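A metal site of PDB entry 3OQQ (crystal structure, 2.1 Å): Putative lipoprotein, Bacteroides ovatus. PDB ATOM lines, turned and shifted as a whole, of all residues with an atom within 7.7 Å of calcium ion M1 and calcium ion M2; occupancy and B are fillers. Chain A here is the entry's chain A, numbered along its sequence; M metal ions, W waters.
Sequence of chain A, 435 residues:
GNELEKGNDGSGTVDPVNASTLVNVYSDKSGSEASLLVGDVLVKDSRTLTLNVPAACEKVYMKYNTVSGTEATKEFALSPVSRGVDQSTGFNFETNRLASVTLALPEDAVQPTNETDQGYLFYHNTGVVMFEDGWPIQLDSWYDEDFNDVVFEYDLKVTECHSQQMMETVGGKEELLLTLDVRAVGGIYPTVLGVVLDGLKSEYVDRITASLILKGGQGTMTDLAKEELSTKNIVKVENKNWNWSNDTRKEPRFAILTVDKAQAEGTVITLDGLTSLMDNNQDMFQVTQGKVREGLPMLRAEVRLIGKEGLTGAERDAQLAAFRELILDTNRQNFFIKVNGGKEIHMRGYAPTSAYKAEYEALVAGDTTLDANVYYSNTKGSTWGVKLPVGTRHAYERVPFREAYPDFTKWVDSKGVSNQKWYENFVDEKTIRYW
Of the 22 residues printed, 3 come within 4 Å of calcium ion M1.
Water W3 bridges the side-chain carboxylate (OE1) of Glu 145 (2.7 Å) and the backbone NH (N) of Asp 146 (3.1 Å).
Of the 22 residues printed, 5 come within 4 Å of calcium ion M2.
OE2 of Glu 132 is bound to calcium ion M1 (2.2 Å).
Water W1 binds calcium ion M1 (2.4 Å).
Water W2 binds calcium ion M1.
Water W3 is bound to calcium ion M1 (2.4 Å).
Calcium ion M1 is bound by OE1 of Glu 132, at 2.5 Å.
OD2 of Asp 149 binds calcium ion M1 (2.5 Å).
OD1 of Asp 146 is bound to calcium ion M1, at 2.5 Å.
Calcium ion M1 is bound by the side-chain carboxylate (OD1) of Asp 149 (2.6 Å).
Calcium ion M1 has eight donor atoms within binding distance.
N of Asp 149 lies within hydrogen-bond range of O of Phe 131.
OD2 of Asp 149 lies close to N of Asp 133 (2.8 Å).
O of Ala 395 sits at hydrogen-bond distance from ND2 of Asn 148, 2.8 Å away.
The backbone NH of Glu 397 is in hydrogen-bond range of the backbone carbonyl oxygen of Val 287, at 2.8 Å.
The side-chain carboxylate of Asp 146 sits close to the backbone NH of Arg 398.
The backbone NH of Phe 147 sits close to the side-chain carboxylate of Glu 132, 2.9 Å away.
Calcium ion M2 is bound by O of Gly 186 (2.4 Å), OD1 of Asn 148 (2.4 Å), OE1 of Glu 397 (2.4 Å), OD2 of Asp 146 (2.4 Å), OD1 of Asp 149 (2.5 Å), OE2 of Glu 397 (2.5 Å), water W1 (2.7 Å) and OD1 of Asp 146 (2.7 Å).
Calcium ion M2 has eight donor atoms within binding distance.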
ATOM      1  N   PHE A 131     -13.903  15.545  27.488  1.00  0.00           N
ATOM      2  CA  PHE A 131     -15.308  15.734  27.135  1.00  0.00           C
ATOM      3  C   PHE A 131     -15.534  15.971  25.677  1.00  0.00           C
ATOM      4  O   PHE A 131     -14.692  16.562  25.009  1.00  0.00           O
ATOM      5  CB  PHE A 131     -15.861  16.962  27.885  1.00  0.00           C
ATOM      6  CG  PHE A 131     -16.539  16.626  29.172  1.00  0.00           C
ATOM      7  CD1 PHE A 131     -17.815  16.075  29.187  1.00  0.00           C
ATOM      8  CD2 PHE A 131     -15.909  16.890  30.382  1.00  0.00           C
ATOM      9  CE1 PHE A 131     -18.449  15.781  30.395  1.00  0.00           C
ATOM     10  CE2 PHE A 131     -16.531  16.564  31.597  1.00  0.00           C
ATOM     11  CZ  PHE A 131     -17.800  16.022  31.591  1.00  0.00           C
ATOM     12  N   GLU A 132     -16.725  15.560  25.210  1.00  0.00           N
ATOM     13  CA  GLU A 132     -17.354  15.851  23.922  1.00  0.00           C
ATOM     14  C   GLU A 132     -18.324  16.996  24.204  1.00  0.00           C
ATOM     15  O   GLU A 132     -18.952  17.010  25.255  1.00  0.00           O
ATOM     16  CB  GLU A 132     -18.050  14.603  23.338  1.00  0.00           C
ATOM     17  CG  GLU A 132     -17.170  13.842  22.354  1.00  0.00           C
ATOM     18  CD  GLU A 132     -16.703  14.690  21.182  1.00  0.00           C
ATOM     19  OE1 GLU A 132     -17.573  15.145  20.417  1.00  0.00           O
ATOM     20  OE2 GLU A 132     -15.473  14.915  21.041  1.00  0.00           O
ATOM     21  N   ASP A 133     -18.436  17.967  23.299  1.00  0.00           N
ATOM     22  CA  ASP A 133     -19.257  19.154  23.523  1.00  0.00           C
ATOM     23  C   ASP A 133     -20.605  19.147  22.811  1.00  0.00           C
ATOM     24  O   ASP A 133     -21.313  20.147  22.861  1.00  0.00           O
ATOM     25  CB  ASP A 133     -18.470  20.406  23.070  1.00  0.00           C
ATOM     26  CG  ASP A 133     -18.014  20.415  21.618  1.00  0.00           C
ATOM     27  OD1 ASP A 133     -18.597  19.683  20.781  1.00  0.00           O
ATOM     28  OD2 ASP A 133     -17.020  21.110  21.316  1.00  0.00           O
ATOM     29  N   GLY A 134     -20.932  18.077  22.120  1.00  0.00           N
ATOM     30  CA  GLY A 134     -22.120  18.018  21.266  1.00  0.00           C
ATOM     31  C   GLY A 134     -23.426  17.568  21.854  1.00  0.00           C
ATOM     32  O   GLY A 134     -24.440  17.674  21.158  1.00  0.00           O
ATOM     33  N   ASP A 144     -16.167   7.379  17.737  1.00  0.00           N
ATOM     34  CA  ASP A 144     -15.633   7.925  16.499  1.00  0.00           C
ATOM     35  C   ASP A 144     -15.470   9.463  16.679  1.00  0.00           C
ATOM     36  O   ASP A 144     -14.889  10.143  15.842  1.00  0.00           O
ATOM     37  CB  ASP A 144     -16.535   7.587  15.299  1.00  0.00           C
ATOM     38  CG  ASP A 144     -16.102   6.332  14.546  1.00  0.00           C
ATOM     39  OD1 ASP A 144     -14.921   5.935  14.677  1.00  0.00           O
ATOM     40  OD2 ASP A 144     -16.914   5.790  13.790  1.00  0.00           O
ATOM     41  N   GLU A 145     -16.004   9.997  17.808  1.00  0.00           N
ATOM     42  CA  GLU A 145     -15.804  11.394  18.225  1.00  0.00           C
ATOM     43  C   GLU A 145     -14.366  11.522  18.671  1.00  0.00           C
ATOM     44  O   GLU A 145     -13.758  10.491  18.981  1.00  0.00           O
ATOM     45  CB  GLU A 145     -16.780  11.799  19.370  1.00  0.00           C
ATOM     46  CG  GLU A 145     -18.270  11.700  19.054  1.00  0.00           C
ATOM     47  CD  GLU A 145     -18.871  12.630  18.012  1.00  0.00           C
ATOM     48  OE1 GLU A 145     -18.113  13.320  17.297  1.00  0.00           O
ATOM     49  OE2 GLU A 145     -20.114  12.631  17.892  1.00  0.00           O
ATOM     50  N   ASP A 146     -13.787  12.753  18.697  1.00  0.00           N
ATOM     51  CA  ASP A 146     -12.382  12.902  19.061  1.00  0.00           C
ATOM     52  C   ASP A 146     -12.112  13.012  20.597  1.00  0.00           C
ATOM     53  O   ASP A 146     -10.967  12.807  21.011  1.00  0.00           O
ATOM     54  CB  ASP A 146     -11.713  14.083  18.287  1.00  0.00           C
ATOM     55  CG  ASP A 146     -12.303  15.484  18.375  1.00  0.00           C
ATOM     56  OD1 ASP A 146     -13.258  15.690  19.171  1.00  0.00           O
ATOM     57  OD2 ASP A 146     -11.826  16.373  17.662  1.00  0.00           O
ATOM     58  N   PHE A 147     -13.143  13.306  21.395  1.00  0.00           N
ATOM     59  CA  PHE A 147     -13.066  13.433  22.869  1.00  0.00           C
ATOM     60  C   PHE A 147     -11.960  14.398  23.332  1.00  0.00           C
ATOM     61  O   PHE A 147     -11.317  14.146  24.350  1.00  0.00           O
ATOM     62  CB  PHE A 147     -12.901  12.055  23.563  1.00  0.00           C
ATOM     63  CG  PHE A 147     -14.239  11.374  23.766  1.00  0.00           C
ATOM     64  CD1 PHE A 147     -14.809  10.610  22.733  1.00  0.00           C
ATOM     65  CD2 PHE A 147     -14.953  11.537  24.944  1.00  0.00           C
ATOM     66  CE1 PHE A 147     -16.064  10.012  22.903  1.00  0.00           C
ATOM     67  CE2 PHE A 147     -16.208  10.939  25.114  1.00  0.00           C
ATOM     68  CZ  PHE A 147     -16.764  10.188  24.092  1.00  0.00           C
ATOM     69  N   ASN A 148     -11.768  15.503  22.618  1.00  0.00           N
ATOM     70  CA  ASN A 148     -10.752  16.471  23.056  1.00  0.00           C
ATOM     71  C   ASN A 148     -11.354  17.878  23.162  1.00  0.00           C
ATOM     72  O   ASN A 148     -10.617  18.849  23.262  1.00  0.00           O
ATOM     73  CB  ASN A 148      -9.545  16.454  22.119  1.00  0.00           C
ATOM     74  CG  ASN A 148      -9.925  16.976  20.751  1.00  0.00           C
ATOM     75  OD1 ASN A 148     -11.044  17.449  20.559  1.00  0.00           O
ATOM     76  ND2 ASN A 148      -9.008  16.936  19.804  1.00  0.00           N
ATOM     77  N   ASP A 149     -12.701  17.981  23.071  1.00  0.00           N
ATOM     78  CA  ASP A 149     -13.420  19.261  23.081  1.00  0.00           C
ATOM     79  C   ASP A 149     -13.094  20.091  24.301  1.00  0.00           C
ATOM     80  O   ASP A 149     -12.961  21.313  24.186  1.00  0.00           O
ATOM     81  CB  ASP A 149     -14.918  19.041  22.902  1.00  0.00           C
ATOM     82  CG  ASP A 149     -15.182  18.277  21.607  1.00  0.00           C
ATOM     83  OD1 ASP A 149     -14.220  18.130  20.785  1.00  0.00           O
ATOM     84  OD2 ASP A 149     -16.308  17.810  21.411  1.00  0.00           O
ATOM     85  N   VAL A 150     -12.919  19.419  25.461  1.00  0.00           N
ATOM     86  CA  VAL A 150     -12.413  19.994  26.694  1.00  0.00           C
ATOM     87  C   VAL A 150     -11.547  18.906  27.318  1.00  0.00           C
ATOM     88  O   VAL A 150     -11.997  17.774  27.531  1.00  0.00           O
ATOM     89  CB  VAL A 150     -13.406  20.606  27.729  1.00  0.00           C
ATOM     90  CG1 VAL A 150     -12.644  21.288  28.868  1.00  0.00           C
ATOM     91  CG2 VAL A 150     -14.369  21.605  27.072  1.00  0.00           C
ATOM     92  N   VAL A 185      -8.649  22.601  24.376  1.00  0.00           N
ATOM     93  CA  VAL A 185     -10.036  22.930  24.068  1.00  0.00           C
ATOM     94  C   VAL A 185     -10.213  22.669  22.557  1.00  0.00           C
ATOM     95  O   VAL A 185      -9.929  23.533  21.734  1.00  0.00           O
ATOM     96  CB  VAL A 185     -10.498  24.343  24.508  1.00  0.00           C
ATOM     97  CG1 VAL A 185     -11.993  24.543  24.258  1.00  0.00           C
ATOM     98  CG2 VAL A 185     -10.178  24.599  25.979  1.00  0.00           C
ATOM     99  N   GLY A 186     -10.626  21.454  22.212  1.00  0.00           N
ATOM    100  CA  GLY A 186     -10.832  21.025  20.828  1.00  0.00           C
ATOM    101  C   GLY A 186     -12.219  21.333  20.312  1.00  0.00           C
ATOM    102  O   GLY A 186     -12.808  20.539  19.599  1.00  0.00           O
ATOM    103  N   GLY A 187     -12.754  22.476  20.701  1.00  0.00           N
ATOM    104  CA  GLY A 187     -14.096  22.852  20.260  1.00  0.00           C
ATOM    105  C   GLY A 187     -14.173  24.348  20.150  1.00  0.00           C
ATOM    106  O   GLY A 187     -13.426  25.039  20.838  1.00  0.00           O
ATOM    107  N   ILE A 188     -15.114  24.824  19.305  1.00  0.00           N
ATOM    108  CA  ILE A 188     -15.341  26.246  19.052  1.00  0.00           C
ATOM    109  C   ILE A 188     -16.206  26.847  20.163  1.00  0.00           C
ATOM    110  O   ILE A 188     -15.960  27.984  20.571  1.00  0.00           O
ATOM    111  CB  ILE A 188     -16.010  26.410  17.642  1.00  0.00           C
ATOM    112  CG1 ILE A 188     -15.024  26.044  16.519  1.00  0.00           C
ATOM    113  CG2 ILE A 188     -16.574  27.812  17.408  1.00  0.00           C
ATOM    114  CD1 ILE A 188     -15.679  25.335  15.323  1.00  0.00           C
ATOM    115  N   MET A 284      -8.197  26.078  17.018  1.00  0.00           N
ATOM    116  CA  MET A 284      -8.648  25.810  18.385  1.00  0.00           C
ATOM    117  C   MET A 284      -7.415  25.730  19.329  1.00  0.00           C
ATOM    118  O   MET A 284      -6.397  26.350  19.013  1.00  0.00           O
ATOM    119  CB  MET A 284      -9.586  24.591  18.443  1.00  0.00           C
ATOM    120  CG  MET A 284     -10.943  24.867  17.736  1.00  0.00           C
ATOM    121  SD  MET A 284     -11.901  23.240  17.317  1.00  0.00           S
ATOM    122  CE  MET A 284     -11.199  22.970  15.633  1.00  0.00           C
ATOM    123  N   VAL A 287      -4.825  21.209  19.964  1.00  0.00           N
ATOM    124  CA  VAL A 287      -5.435  20.023  19.306  1.00  0.00           C
ATOM    125  C   VAL A 287      -5.043  19.864  17.803  1.00  0.00           C
ATOM    126  O   VAL A 287      -5.294  18.805  17.190  1.00  0.00           O
ATOM    127  CB  VAL A 287      -7.001  19.997  19.467  1.00  0.00           C
ATOM    128  CG1 VAL A 287      -7.421  19.914  20.924  1.00  0.00           C
ATOM    129  CG2 VAL A 287      -7.697  21.176  18.750  1.00  0.00           C
ATOM    130  N   ALA A 395      -6.483  13.096  21.740  1.00  0.00           N
ATOM    131  CA  ALA A 395      -6.409  12.962  20.289  1.00  0.00           C
ATOM    132  C   ALA A 395      -6.262  14.290  19.581  1.00  0.00           C
ATOM    133  O   ALA A 395      -6.772  15.321  20.044  1.00  0.00           O
ATOM    134  CB  ALA A 395      -7.676  12.293  19.777  1.00  0.00           C
ATOM    135  N   TYR A 396      -5.652  14.236  18.378  1.00  0.00           N
ATOM    136  CA  TYR A 396      -5.575  15.385  17.461  1.00  0.00           C
ATOM    137  C   TYR A 396      -6.997  15.673  16.994  1.00  0.00           C
ATOM    138  O   TYR A 396      -7.837  14.768  17.009  1.00  0.00           O
ATOM    139  CB  TYR A 396      -4.679  15.068  16.241  1.00  0.00           C
ATOM    140  CG  TYR A 396      -3.204  15.231  16.508  1.00  0.00           C
ATOM    141  CD1 TYR A 396      -2.637  16.503  16.653  1.00  0.00           C
ATOM    142  CD2 TYR A 396      -2.351  14.135  16.541  1.00  0.00           C
ATOM    143  CE1 TYR A 396      -1.283  16.663  16.916  1.00  0.00           C
ATOM    144  CE2 TYR A 396      -0.988  14.292  16.777  1.00  0.00           C
ATOM    145  CZ  TYR A 396      -0.458  15.557  16.978  1.00  0.00           C
ATOM    146  OH  TYR A 396       0.881  15.718  17.212  1.00  0.00           O
ATOM    147  N   GLU A 397      -7.289  16.924  16.622  1.00  0.00           N
ATOM    148  CA  GLU A 397      -8.625  17.333  16.180  1.00  0.00           C
ATOM    149  C   GLU A 397      -9.161  16.449  15.058  1.00  0.00           C
ATOM    150  O   GLU A 397      -8.439  16.167  14.090  1.00  0.00           O
ATOM    151  CB  GLU A 397      -8.638  18.804  15.748  1.00  0.00           C
ATOM    152  CG  GLU A 397     -10.034  19.420  15.693  1.00  0.00           C
ATOM    153  CD  GLU A 397     -10.957  19.272  16.898  1.00  0.00           C
ATOM    154  OE1 GLU A 397     -10.462  19.020  18.023  1.00  0.00           O
ATOM    155  OE2 GLU A 397     -12.185  19.430  16.708  1.00  0.00           O
ATOM    156  N   ARG A 398     -10.434  16.009  15.214  1.00  0.00           N
ATOM    157  CA  ARG A 398     -11.203  15.159  14.285  1.00  0.00           C
ATOM    158  C   ARG A 398     -10.628  13.743  14.118  1.00  0.00           C
ATOM    159  O   ARG A 398     -11.084  12.999  13.266  1.00  0.00           O
ATOM    160  CB  ARG A 398     -11.378  15.835  12.914  1.00  0.00           C
ATOM    161  CG  ARG A 398     -12.442  16.971  12.923  1.00  0.00           C
ATOM    162  CD  ARG A 398     -12.496  17.706  11.587  1.00  0.00           C
ATOM    163  NE  ARG A 398     -11.198  18.277  11.224  1.00  0.00           N
ATOM    164  CZ  ARG A 398     -10.766  19.488  11.607  1.00  0.00           C
ATOM    165  NH1 ARG A 398     -11.556  20.284  12.326  1.00  0.00           N
ATOM    166  NH2 ARG A 398      -9.566  19.905  11.255  1.00  0.00           N
ATOM    167  N   VAL A 399      -9.665  13.348  14.962  1.00  0.00           N
ATOM    168  CA  VAL A 399      -9.170  11.966  14.937  1.00  0.00           C
ATOM    169  C   VAL A 399     -10.116  11.136  15.833  1.00  0.00           C
ATOM    170  O   VAL A 399     -10.265  11.466  17.012  1.00  0.00           O
ATOM    171  CB  VAL A 399      -7.677  11.839  15.382  1.00  0.00           C
ATOM    172  CG1 VAL A 399      -7.312  10.374  15.628  1.00  0.00           C
ATOM    173  CG2 VAL A 399      -6.735  12.469  14.369  1.00  0.00           C
HETATM  174 CA    CA M   1     -15.670  16.388  19.430  1.00  0.00          CA
HETATM  175 CA    CA M   2     -12.570  18.289  18.931  1.00  0.00          CA
HETATM  176  O   HOH W   1     -15.022  18.060  17.892  1.00  0.00           O
HETATM  177  O   HOH W   2     -17.615  17.568  18.719  1.00  0.00           O
HETATM  178  O   HOH W   3     -15.876  14.779  17.639  1.00  0.00           O
